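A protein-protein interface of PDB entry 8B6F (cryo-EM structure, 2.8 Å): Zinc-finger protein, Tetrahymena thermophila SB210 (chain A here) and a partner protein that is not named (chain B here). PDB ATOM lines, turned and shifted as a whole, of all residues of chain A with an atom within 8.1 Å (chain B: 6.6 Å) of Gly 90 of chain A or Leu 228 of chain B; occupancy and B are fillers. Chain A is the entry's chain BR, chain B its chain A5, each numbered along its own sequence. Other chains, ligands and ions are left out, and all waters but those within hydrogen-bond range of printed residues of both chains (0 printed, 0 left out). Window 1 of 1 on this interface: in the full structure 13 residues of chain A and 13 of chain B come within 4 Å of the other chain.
O of Thr 91 of chain A lies close to OD1 of Asp 229 of chain B.
The backbone carbonyl oxygen of Tyr 79 of chain A sits at hydrogen-bond distance from the side-chain amide nitrogen of Asn 236 of chain B.
The backbone NH (N) of Asp 229 of chain B sits at hydrogen-bond distance from the backbone carbonyl oxygen (O) of Gly 90 of chain A, at 3.3 Å.
The backbone carbonyl oxygen of Phe 224 of chain B sits at hydrogen-bond distance from the side-chain hydroxyl of Thr 91 of chain A, at 2.5 Å.
The guanidinium group of Arg 86 of chain A lies within salt-bridge range of the side-chain carboxylate of Asp 229 of chain B (3.5 Å).
OG of Ser 231 of chain B lies within hydrogen-bond range of NH2 of Arg 86 of chain A, 3.5 Å away.
The side-chain hydroxyl (OH) of Tyr 122 of chain A sits close to the side-chain sulfur (SG) of Cys 87 of chain A (3.3 Å).
O of Ile 88 of chain A lies within hydrogen-bond range of N of His 97 of chain A, at 3.0 Å.
The backbone NH (N) of Ala 227 of chain B sits at hydrogen-bond distance from the side-chain amide oxygen (OE1) of Gln 241 of chain B (2.9 Å).
The side-chain carboxylate (OD1) of Asp 229 of chain B lies close to the side-chain amide oxygen (OD1) of Asn 230 of chain B (2.7 Å).
OG of Ser 231 of chain B sits at hydrogen-bond distance from OD2 of Asp 229 of chain B (3.4 Å).
Among the printed residues, pairs that only touch across the chains: Arg 86 of chain A with Phe 232 of chain B (3.2 Å), Ile 78 of chain A with Val 240 of chain B (3.5 Å), Val 85 of chain A with Phe 232 of chain B (3.5 Å), Thr 91 of chain A with Gln 226 of chain B (3.6 Å), Ala 95 of chain A with Trp 225 of chain B (3.6 Å), Tyr 122 of chain A with Phe 232 of chain B (3.6 Å), Thr 91 of chain A with Leu 228 of chain B (3.6 Å), Gly 90 of chain A with Leu 228 of chain B (3.6 Å), Ile 78 of chain A with Asn 236 of chain B (3.6 Å), Glu 92 of chain A with Phe 224 of chain B (3.7 Å), Gly 90 of chain A with Ala 227 of chain B (3.7 Å), Ala 95 of chain A with Phe 224 of chain B (3.8 Å), Ile 88 of chain A with Asp 229 of chain B (3.8 Å), Gly 90 of chain A with Gln 226 of chain B (3.8 Å), Ile 78 of chain A with Leu 228 of chain B (3.9 Å) and Tyr 122 of chain A with Leu 228 of chain B (3.96 Å).
Gly 90 of chain A touches four residues of chain B.
Leu 228 of chain B touches just these residues of chain A: Ile 78, Gly 90, Thr 91 and Tyr 122.
Of chain A, only Gly 90 comes within 4 Å of Ala 227 of chain B.
Of the printed residues of chain B, Ile 88 of chain A touches Asp 229.
Printed residues of chain A within 4 Å of Gln 226 of chain B: Gly 90 and Thr 91.
Of the printed residues of chain B, Thr 91 of chain A touches Phe 224 (2.5 Å), Gln 226 (3.6 Å), Leu 228 (3.6 Å) and Asp 229 (3.3 Å).
Gly 89 of chain A touches none of the printed residues of chain B.
Val 75 of chain A touches none of the printed residues of chain B.
The nearest residue of chain A that does not touch Leu 228 of chain B is Leu 120 of chain A (4.1 Å).
The nearest printed residue of chain A that does not touch Trp 225 of chain B is Thr 91 of chain A (4.6 Å).
Hydrophobic or aromatic side chains of chain B within 4 Å of the printed part of chain A: Phe 224, Trp 225, Leu 228, Phe 232 and Val 240.
Of the 20 printed residues of chain A, 10 touch a printed residue of chain B.
Among the printed residues, 22 pairs touch across the chains.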
ATOM      1  N   VAL A  75     -11.276  29.563 -27.304  1.00  0.00           N
ATOM      2  CA  VAL A  75     -12.356  28.925 -28.065  1.00  0.00           C
ATOM      3  C   VAL A  75     -12.234  29.321 -29.534  1.00  0.00           C
ATOM      4  O   VAL A  75     -12.142  30.525 -29.844  1.00  0.00           O
ATOM      5  CB  VAL A  75     -13.728  29.327 -27.498  1.00  0.00           C
ATOM      6  CG1 VAL A  75     -14.848  28.633 -28.262  1.00  0.00           C
ATOM      7  CG2 VAL A  75     -13.810  28.998 -26.015  1.00  0.00           C
ATOM      8  N   ILE A  78     -16.707  29.351 -34.340  1.00  0.00           N
ATOM      9  CA  ILE A  78     -17.767  28.377 -34.573  1.00  0.00           C
ATOM     10  C   ILE A  78     -18.363  28.658 -35.945  1.00  0.00           C
ATOM     11  O   ILE A  78     -18.818  29.775 -36.214  1.00  0.00           O
ATOM     12  CB  ILE A  78     -18.839  28.443 -33.477  1.00  0.00           C
ATOM     13  CG1 ILE A  78     -18.198  28.274 -32.096  1.00  0.00           C
ATOM     14  CG2 ILE A  78     -19.895  27.371 -33.701  1.00  0.00           C
ATOM     15  CD1 ILE A  78     -19.122  28.607 -30.948  1.00  0.00           C
ATOM     16  N   TYR A  79     -18.364  27.653 -36.813  1.00  0.00           N
ATOM     17  CA  TYR A  79     -18.827  27.805 -38.186  1.00  0.00           C
ATOM     18  C   TYR A  79     -20.277  27.347 -38.281  1.00  0.00           C
ATOM     19  O   TYR A  79     -20.594  26.201 -37.943  1.00  0.00           O
ATOM     20  CB  TYR A  79     -17.937  27.021 -39.146  1.00  0.00           C
ATOM     21  CG  TYR A  79     -16.537  27.582 -39.225  1.00  0.00           C
ATOM     22  CD1 TYR A  79     -16.243  28.653 -40.059  1.00  0.00           C
ATOM     23  CD2 TYR A  79     -15.515  27.053 -38.451  1.00  0.00           C
ATOM     24  CE1 TYR A  79     -14.966  29.175 -40.127  1.00  0.00           C
ATOM     25  CE2 TYR A  79     -14.234  27.568 -38.510  1.00  0.00           C
ATOM     26  CZ  TYR A  79     -13.966  28.628 -39.350  1.00  0.00           C
ATOM     27  OH  TYR A  79     -12.692  29.143 -39.412  1.00  0.00           O
ATOM     28  N   VAL A  80     -21.148  28.241 -38.743  1.00  0.00           N
ATOM     29  CA  VAL A  80     -22.586  28.009 -38.799  1.00  0.00           C
ATOM     30  C   VAL A  80     -23.036  28.140 -40.247  1.00  0.00           C
ATOM     31  O   VAL A  80     -22.668  29.100 -40.933  1.00  0.00           O
ATOM     32  CB  VAL A  80     -23.353  28.994 -37.897  1.00  0.00           C
ATOM     33  CG1 VAL A  80     -24.840  28.682 -37.906  1.00  0.00           C
ATOM     34  CG2 VAL A  80     -22.806  28.955 -36.480  1.00  0.00           C
ATOM     35  N   VAL A  85     -27.336  33.549 -36.909  1.00  0.00           N
ATOM     36  CA  VAL A  85     -27.108  32.591 -35.836  1.00  0.00           C
ATOM     37  C   VAL A  85     -27.723  33.133 -34.555  1.00  0.00           C
ATOM     38  O   VAL A  85     -27.583  34.318 -34.237  1.00  0.00           O
ATOM     39  CB  VAL A  85     -25.606  32.294 -35.643  1.00  0.00           C
ATOM     40  CG1 VAL A  85     -24.843  33.562 -35.300  1.00  0.00           C
ATOM     41  CG2 VAL A  85     -25.405  31.237 -34.566  1.00  0.00           C
ATOM     42  N   ARG A  86     -28.409  32.259 -33.827  1.00  0.00           N
ATOM     43  CA  ARG A  86     -29.049  32.600 -32.564  1.00  0.00           C
ATOM     44  C   ARG A  86     -28.168  32.124 -31.418  1.00  0.00           C
ATOM     45  O   ARG A  86     -27.717  30.974 -31.413  1.00  0.00           O
ATOM     46  CB  ARG A  86     -30.435  31.964 -32.470  1.00  0.00           C
ATOM     47  CG  ARG A  86     -31.199  32.305 -31.200  1.00  0.00           C
ATOM     48  CD  ARG A  86     -32.452  31.454 -31.080  1.00  0.00           C
ATOM     49  NE  ARG A  86     -32.139  30.045 -30.881  1.00  0.00           N
ATOM     50  CZ  ARG A  86     -33.036  29.069 -30.889  1.00  0.00           C
ATOM     51  NH1 ARG A  86     -34.318  29.311 -31.106  1.00  0.00           N
ATOM     52  NH2 ARG A  86     -32.637  27.820 -30.679  1.00  0.00           N
ATOM     53  N   CYS A  87     -27.925  33.007 -30.452  1.00  0.00           N
ATOM     54  CA  CYS A  87     -27.098  32.695 -29.295  1.00  0.00           C
ATOM     55  C   CYS A  87     -27.881  32.989 -28.026  1.00  0.00           C
ATOM     56  O   CYS A  87     -28.483  34.060 -27.898  1.00  0.00           O
ATOM     57  CB  CYS A  87     -25.803  33.519 -29.323  1.00  0.00           C
ATOM     58  SG  CYS A  87     -24.592  33.119 -28.041  1.00  0.00           S
ATOM     59  N   ILE A  88     -27.874  32.037 -27.094  1.00  0.00           N
ATOM     60  CA  ILE A  88     -28.475  32.212 -25.778  1.00  0.00           C
ATOM     61  C   ILE A  88     -27.474  32.000 -24.654  1.00  0.00           C
ATOM     62  O   ILE A  88     -27.850  32.090 -23.482  1.00  0.00           O
ATOM     63  CB  ILE A  88     -29.692  31.285 -25.584  1.00  0.00           C
ATOM     64  CG1 ILE A  88     -29.277  29.816 -25.715  1.00  0.00           C
ATOM     65  CG2 ILE A  88     -30.777  31.634 -26.592  1.00  0.00           C
ATOM     66  CD1 ILE A  88     -30.392  28.827 -25.427  1.00  0.00           C
ATOM     67  N   GLY A  89     -26.216  31.714 -24.973  1.00  0.00           N
ATOM     68  CA  GLY A  89     -25.205  31.536 -23.943  1.00  0.00           C
ATOM     69  C   GLY A  89     -25.459  30.349 -23.042  1.00  0.00           C
ATOM     70  O   GLY A  89     -25.228  30.432 -21.830  1.00  0.00           O
ATOM     71  N   GLY A  90     -25.929  29.242 -23.605  1.00  0.00           N
ATOM     72  CA  GLY A  90     -26.193  28.062 -22.806  1.00  0.00           C
ATOM     73  C   GLY A  90     -27.020  27.062 -23.587  1.00  0.00           C
ATOM     74  O   GLY A  90     -27.102  27.126 -24.814  1.00  0.00           O
ATOM     75  N   THR A  91     -27.630  26.135 -22.849  1.00  0.00           N
ATOM     76  CA  THR A  91     -28.448  25.090 -23.445  1.00  0.00           C
ATOM     77  C   THR A  91     -29.940  25.389 -23.391  1.00  0.00           C
ATOM     78  O   THR A  91     -30.703  24.781 -24.148  1.00  0.00           O
ATOM     79  CB  THR A  91     -28.190  23.750 -22.744  1.00  0.00           C
ATOM     80  OG1 THR A  91     -28.532  23.857 -21.356  1.00  0.00           O
ATOM     81  CG2 THR A  91     -26.733  23.359 -22.869  1.00  0.00           C
ATOM     82  N   GLU A  92     -30.368  26.306 -22.528  1.00  0.00           N
ATOM     83  CA  GLU A  92     -31.783  26.593 -22.354  1.00  0.00           C
ATOM     84  C   GLU A  92     -31.955  28.059 -21.984  1.00  0.00           C
ATOM     85  O   GLU A  92     -31.038  28.701 -21.466  1.00  0.00           O
ATOM     86  CB  GLU A  92     -32.399  25.691 -21.279  1.00  0.00           C
ATOM     87  CG  GLU A  92     -33.848  26.003 -20.948  1.00  0.00           C
ATOM     88  CD  GLU A  92     -34.449  24.999 -19.992  1.00  0.00           C
ATOM     89  OE1 GLU A  92     -34.191  23.788 -20.157  1.00  0.00           O
ATOM     90  OE2 GLU A  92     -35.159  25.423 -19.058  1.00  0.00           O
ATOM     91  N   ILE A  93     -33.151  28.582 -22.260  1.00  0.00           N
ATOM     92  CA  ILE A  93     -33.456  29.960 -21.905  1.00  0.00           C
ATOM     93  C   ILE A  93     -33.347  30.130 -20.398  1.00  0.00           C
ATOM     94  O   ILE A  93     -33.698  29.234 -19.621  1.00  0.00           O
ATOM     95  CB  ILE A  93     -34.855  30.350 -22.414  1.00  0.00           C
ATOM     96  CG1 ILE A  93     -34.893  30.347 -23.945  1.00  0.00           C
ATOM     97  CG2 ILE A  93     -35.278  31.713 -21.867  1.00  0.00           C
ATOM     98  CD1 ILE A  93     -34.032  31.410 -24.604  1.00  0.00           C
ATOM     99  N   ASN A  94     -32.848  31.290 -19.979  1.00  0.00           N
ATOM    100  CA  ASN A  94     -32.658  31.694 -18.593  1.00  0.00           C
ATOM    101  C   ASN A  94     -31.416  31.054 -17.986  1.00  0.00           C
ATOM    102  O   ASN A  94     -31.101  31.344 -16.829  1.00  0.00           O
ATOM    103  CB  ASN A  94     -33.872  31.361 -17.711  1.00  0.00           C
ATOM    104  CG  ASN A  94     -33.961  32.243 -16.484  1.00  0.00           C
ATOM    105  OD1 ASN A  94     -34.883  33.047 -16.353  1.00  0.00           O
ATOM    106  ND2 ASN A  94     -33.007  32.094 -15.573  1.00  0.00           N
ATOM    107  N   ALA A  95     -30.703  30.196 -18.715  1.00  0.00           N
ATOM    108  CA  ALA A  95     -29.454  29.616 -18.241  1.00  0.00           C
ATOM    109  C   ALA A  95     -28.229  30.336 -18.784  1.00  0.00           C
ATOM    110  O   ALA A  95     -27.104  29.947 -18.460  1.00  0.00           O
ATOM    111  CB  ALA A  95     -29.386  28.133 -18.618  1.00  0.00           C
ATOM    112  N   GLY A  96     -28.420  31.372 -19.595  1.00  0.00           N
ATOM    113  CA  GLY A  96     -27.318  32.133 -20.147  1.00  0.00           C
ATOM    114  C   GLY A  96     -27.655  33.604 -20.224  1.00  0.00           C
ATOM    115  O   GLY A  96     -28.131  34.185 -19.246  1.00  0.00           O
ATOM    116  N   HIS A  97     -27.420  34.216 -21.371  1.00  0.00           N
ATOM    117  CA  HIS A  97     -27.761  35.608 -21.614  1.00  0.00           C
ATOM    118  C   HIS A  97     -29.024  35.705 -22.454  1.00  0.00           C
ATOM    119  O   HIS A  97     -29.493  34.713 -23.017  1.00  0.00           O
ATOM    120  CB  HIS A  97     -26.595  36.318 -22.302  1.00  0.00           C
ATOM    121  CG  HIS A  97     -26.270  35.778 -23.659  1.00  0.00           C
ATOM    122  ND1 HIS A  97     -27.091  35.960 -24.752  1.00  0.00           N
ATOM    123  CD2 HIS A  97     -25.203  35.076 -24.105  1.00  0.00           C
ATOM    124  CE1 HIS A  97     -26.547  35.387 -25.808  1.00  0.00           C
ATOM    125  NE2 HIS A  97     -25.400  34.845 -25.444  1.00  0.00           N
ATOM    126  N   CYS A 118     -21.418  37.218 -24.714  1.00  0.00           N
ATOM    127  CA  CYS A 118     -20.299  36.310 -24.513  1.00  0.00           C
ATOM    128  C   CYS A 118     -19.358  36.435 -25.701  1.00  0.00           C
ATOM    129  O   CYS A 118     -19.768  36.814 -26.799  1.00  0.00           O
ATOM    130  CB  CYS A 118     -20.752  34.851 -24.335  1.00  0.00           C
ATOM    131  SG  CYS A 118     -21.814  34.204 -25.639  1.00  0.00           S
ATOM    132  N   LEU A 120     -18.018  34.363 -27.642  1.00  0.00           N
ATOM    133  CA  LEU A 120     -18.054  33.371 -28.709  1.00  0.00           C
ATOM    134  C   LEU A 120     -18.146  34.056 -30.065  1.00  0.00           C
ATOM    135  O   LEU A 120     -18.955  34.967 -30.263  1.00  0.00           O
ATOM    136  CB  LEU A 120     -19.239  32.427 -28.513  1.00  0.00           C
ATOM    137  CG  LEU A 120     -19.158  31.458 -27.333  1.00  0.00           C
ATOM    138  CD1 LEU A 120     -20.441  30.658 -27.218  1.00  0.00           C
ATOM    139  CD2 LEU A 120     -17.967  30.525 -27.479  1.00  0.00           C
ATOM    140  N   TYR A 122     -18.698  33.612 -34.159  1.00  0.00           N
ATOM    141  CA  TYR A 122     -19.334  32.771 -35.159  1.00  0.00           C
ATOM    142  C   TYR A 122     -19.014  33.292 -36.553  1.00  0.00           C
ATOM    143  O   TYR A 122     -18.939  34.504 -36.771  1.00  0.00           O
ATOM    144  CB  TYR A 122     -20.852  32.741 -34.967  1.00  0.00           C
ATOM    145  CG  TYR A 122     -21.295  32.347 -33.578  1.00  0.00           C
ATOM    146  CD1 TYR A 122     -21.480  31.015 -33.238  1.00  0.00           C
ATOM    147  CD2 TYR A 122     -21.540  33.312 -32.611  1.00  0.00           C
ATOM    148  CE1 TYR A 122     -21.889  30.654 -31.971  1.00  0.00           C
ATOM    149  CE2 TYR A 122     -21.948  32.962 -31.341  1.00  0.00           C
ATOM    150  CZ  TYR A 122     -22.122  31.631 -31.026  1.00  0.00           C
ATOM    151  OH  TYR A 122     -22.530  31.275 -29.762  1.00  0.00           O
ATOM    152  N   PHE B 224     -26.374  20.009 -18.488  1.00  0.00           N
ATOM    153  CA  PHE B 224     -27.267  21.148 -18.650  1.00  0.00           C
ATOM    154  C   PHE B 224     -26.503  22.446 -18.874  1.00  0.00           C
ATOM    155  O   PHE B 224     -27.084  23.416 -19.375  1.00  0.00           O
ATOM    156  CB  PHE B 224     -28.165  21.275 -17.418  1.00  0.00           C
ATOM    157  CG  PHE B 224     -29.089  22.459 -17.453  1.00  0.00           C
ATOM    158  CD1 PHE B 224     -30.340  22.360 -18.037  1.00  0.00           C
ATOM    159  CD2 PHE B 224     -28.712  23.666 -16.887  1.00  0.00           C
ATOM    160  CE1 PHE B 224     -31.195  23.445 -18.064  1.00  0.00           C
ATOM    161  CE2 PHE B 224     -29.562  24.754 -16.911  1.00  0.00           C
ATOM    162  CZ  PHE B 224     -30.805  24.644 -17.500  1.00  0.00           C
ATOM    163  N   TRP B 225     -25.218  22.488 -18.517  1.00  0.00           N
ATOM    164  CA  TRP B 225     -24.405  23.693 -18.619  1.00  0.00           C
ATOM    165  C   TRP B 225     -23.405  23.620 -19.767  1.00  0.00           C
ATOM    166  O   TRP B 225     -22.294  24.141 -19.661  1.00  0.00           O
ATOM    167  CB  TRP B 225     -23.674  23.949 -17.302  1.00  0.00           C
ATOM    168  CG  TRP B 225     -24.592  24.189 -16.154  1.00  0.00           C
ATOM    169  CD1 TRP B 225     -24.930  23.301 -15.177  1.00  0.00           C
ATOM    170  CD2 TRP B 225     -25.300  25.397 -15.863  1.00  0.00           C
ATOM    171  NE1 TRP B 225     -25.803  23.883 -14.293  1.00  0.00           N
ATOM    172  CE2 TRP B 225     -26.048  25.170 -14.692  1.00  0.00           C
ATOM    173  CE3 TRP B 225     -25.375  26.650 -16.478  1.00  0.00           C
ATOM    174  CZ2 TRP B 225     -26.858  26.149 -14.122  1.00  0.00           C
ATOM    175  CZ3 TRP B 225     -26.179  27.621 -15.914  1.00  0.00           C
ATOM    176  CH2 TRP B 225     -26.911  27.366 -14.746  1.00  0.00           C
ATOM    177  N   GLN B 226     -23.779  22.978 -20.870  1.00  0.00           N
ATOM    178  CA  GLN B 226     -22.918  22.962 -22.041  1.00  0.00           C
ATOM    179  C   GLN B 226     -22.808  24.360 -22.639  1.00  0.00           C
ATOM    180  O   GLN B 226     -23.699  25.198 -22.491  1.00  0.00           O
ATOM    181  CB  GLN B 226     -23.453  21.989 -23.089  1.00  0.00           C
ATOM    182  CG  GLN B 226     -23.187  20.530 -22.768  1.00  0.00           C
ATOM    183  CD  GLN B 226     -23.633  19.597 -23.878  1.00  0.00           C
ATOM    184  OE1 GLN B 226     -22.958  18.616 -24.184  1.00  0.00           O
ATOM    185  NE2 GLN B 226     -24.780  19.894 -24.482  1.00  0.00           N
ATOM    186  N   ALA B 227     -21.685  24.610 -23.314  1.00  0.00           N
ATOM    187  CA  ALA B 227     -21.447  25.935 -23.877  1.00  0.00           C
ATOM    188  C   ALA B 227     -22.482  26.282 -24.940  1.00  0.00           C
ATOM    189  O   ALA B 227     -22.985  27.410 -24.979  1.00  0.00           O
ATOM    190  CB  ALA B 227     -20.037  26.006 -24.462  1.00  0.00           C
ATOM    191  N   LEU B 228     -22.814  25.330 -25.809  1.00  0.00           N
ATOM    192  CA  LEU B 228     -23.684  25.577 -26.948  1.00  0.00           C
ATOM    193  C   LEU B 228     -25.025  24.878 -26.779  1.00  0.00           C
ATOM    194  O   LEU B 228     -25.144  23.874 -26.071  1.00  0.00           O
ATOM    195  CB  LEU B 228     -23.040  25.116 -28.260  1.00  0.00           C
ATOM    196  CG  LEU B 228     -21.873  25.940 -28.811  1.00  0.00           C
ATOM    197  CD1 LEU B 228     -21.414  25.345 -30.129  1.00  0.00           C
ATOM    198  CD2 LEU B 228     -22.243  27.402 -28.985  1.00  0.00           C
ATOM    199  N   ASP B 229     -26.035  25.429 -27.448  1.00  0.00           N
ATOM    200  CA  ASP B 229     -27.370  24.862 -27.465  1.00  0.00           C
ATOM    201  C   ASP B 229     -27.452  23.716 -28.471  1.00  0.00           C
ATOM    202  O   ASP B 229     -26.637  23.599 -29.389  1.00  0.00           O
ATOM    203  CB  ASP B 229     -28.387  25.947 -27.820  1.00  0.00           C
ATOM    204  CG  ASP B 229     -29.810  25.452 -27.775  1.00  0.00           C
ATOM    205  OD1 ASP B 229     -30.028  24.301 -27.341  1.00  0.00           O
ATOM    206  OD2 ASP B 229     -30.716  26.212 -28.175  1.00  0.00           O
ATOM    207  N   ASN B 230     -28.461  22.859 -28.287  1.00  0.00           N
ATOM    208  CA  ASN B 230     -28.652  21.740 -29.203  1.00  0.00           C
ATOM    209  C   ASN B 230     -28.993  22.203 -30.613  1.00  0.00           C
ATOM    210  O   ASN B 230     -28.774  21.452 -31.569  1.00  0.00           O
ATOM    211  CB  ASN B 230     -29.744  20.803 -28.682  1.00  0.00           C
ATOM    212  CG  ASN B 230     -31.089  21.488 -28.551  1.00  0.00           C
ATOM    213  OD1 ASN B 230     -31.283  22.604 -29.030  1.00  0.00           O
ATOM    214  ND2 ASN B 230     -32.031  20.813 -27.905  1.00  0.00           N
ATOM    215  N   SER B 231     -29.525  23.417 -30.766  1.00  0.00           N
ATOM    216  CA  SER B 231     -29.836  23.928 -32.096  1.00  0.00           C
ATOM    217  C   SER B 231     -28.595  24.032 -32.969  1.00  0.00           C
ATOM    218  O   SER B 231     -28.714  24.027 -34.199  1.00  0.00           O
ATOM    219  CB  SER B 231     -30.516  25.295 -31.993  1.00  0.00           C
ATOM    220  OG  SER B 231     -29.647  26.258 -31.427  1.00  0.00           O
ATOM    221  N   PHE B 232     -27.415  24.129 -32.367  1.00  0.00           N
ATOM    222  CA  PHE B 232     -26.176  24.153 -33.122  1.00  0.00           C
ATOM    223  C   PHE B 232     -25.843  22.755 -33.633  1.00  0.00           C
ATOM    224  O   PHE B 232     -26.405  21.748 -33.196  1.00  0.00           O
ATOM    225  CB  PHE B 232     -25.033  24.693 -32.264  1.00  0.00           C
ATOM    226  CG  PHE B 232     -25.142  26.160 -31.966  1.00  0.00           C
ATOM    227  CD1 PHE B 232     -25.830  26.605 -30.849  1.00  0.00           C
ATOM    228  CD2 PHE B 232     -24.556  27.093 -32.804  1.00  0.00           C
ATOM    229  CE1 PHE B 232     -25.932  27.953 -30.574  1.00  0.00           C
ATOM    230  CE2 PHE B 232     -24.654  28.442 -32.534  1.00  0.00           C
ATOM    231  CZ  PHE B 232     -25.344  28.874 -31.417  1.00  0.00           C
ATOM    232  N   SER B 233     -24.911  22.702 -34.575  1.00  0.00           N
ATOM    233  CA  SER B 233     -24.514  21.427 -35.147  1.00  0.00           C
ATOM    234  C   SER B 233     -23.851  20.561 -34.078  1.00  0.00           C
ATOM    235  O   SER B 233     -23.147  21.083 -33.206  1.00  0.00           O
ATOM    236  CB  SER B 233     -23.548  21.646 -36.312  1.00  0.00           C
ATOM    237  OG  SER B 233     -23.117  20.411 -36.855  1.00  0.00           O
ATOM    238  N   ASN B 236     -20.191  21.296 -34.078  1.00  0.00           N
ATOM    239  CA  ASN B 236     -19.853  22.537 -33.389  1.00  0.00           C
ATOM    240  C   ASN B 236     -19.904  22.357 -31.878  1.00  0.00           C
ATOM    241  O   ASN B 236     -19.025  22.847 -31.158  1.00  0.00           O
ATOM    242  CB  ASN B 236     -20.802  23.656 -33.823  1.00  0.00           C
ATOM    243  CG  ASN B 236     -20.539  24.131 -35.236  1.00  0.00           C
ATOM    244  OD1 ASN B 236     -19.402  24.122 -35.705  1.00  0.00           O
ATOM    245  ND2 ASN B 236     -21.593  24.552 -35.925  1.00  0.00           N
ATOM    246  N   ILE B 237     -20.922  21.658 -31.376  1.00  0.00           N
ATOM    247  CA  ILE B 237     -21.031  21.440 -29.935  1.00  0.00           C
ATOM    248  C   ILE B 237     -19.817  20.673 -29.428  1.00  0.00           C
ATOM    249  O   ILE B 237     -19.203  21.040 -28.420  1.00  0.00           O
ATOM    250  CB  ILE B 237     -22.342  20.707 -29.600  1.00  0.00           C
ATOM    251  CG1 ILE B 237     -23.541  21.584 -29.968  1.00  0.00           C
ATOM    252  CG2 ILE B 237     -22.387  20.340 -28.118  1.00  0.00           C
ATOM    253  CD1 ILE B 237     -24.876  20.883 -29.855  1.00  0.00           C
ATOM    254  N   ALA B 238     -19.455  19.595 -30.120  1.00  0.00           N
ATOM    255  CA  ALA B 238     -18.305  18.802 -29.697  1.00  0.00           C
ATOM    256  C   ALA B 238     -17.021  19.616 -29.758  1.00  0.00           C
ATOM    257  O   ALA B 238     -16.175  19.525 -28.861  1.00  0.00           O
ATOM    258  CB  ALA B 238     -18.188  17.547 -30.561  1.00  0.00           C
ATOM    259  N   VAL B 240     -16.634  22.920 -29.474  1.00  0.00           N
ATOM    260  CA  VAL B 240     -16.590  23.904 -28.396  1.00  0.00           C
ATOM    261  C   VAL B 240     -16.295  23.226 -27.066  1.00  0.00           C
ATOM    262  O   VAL B 240     -15.500  23.726 -26.260  1.00  0.00           O
ATOM    263  CB  VAL B 240     -17.904  24.705 -28.347  1.00  0.00           C
ATOM    264  CG1 VAL B 240     -17.975  25.565 -27.090  1.00  0.00           C
ATOM    265  CG2 VAL B 240     -18.025  25.576 -29.580  1.00  0.00           C
ATOM    266  N   GLN B 241     -16.926  22.080 -26.811  1.00  0.00           N
ATOM    267  CA  GLN B 241     -16.677  21.367 -25.564  1.00  0.00           C
ATOM    268  C   GLN B 241     -15.222  20.928 -25.466  1.00  0.00           C
ATOM    269  O   GLN B 241     -14.597  21.055 -24.407  1.00  0.00           O
ATOM    270  CB  GLN B 241     -17.615  20.167 -25.455  1.00  0.00           C
ATOM    271  CG  GLN B 241     -19.083  20.553 -25.337  1.00  0.00           C
ATOM    272  CD  GLN B 241     -19.392  21.281 -24.045  1.00  0.00           C
ATOM    273  OE1 GLN B 241     -19.974  22.363 -24.053  1.00  0.00           O
ATOM    274  NE2 GLN B 241     -19.008  20.682 -22.923  1.00  0.00           N
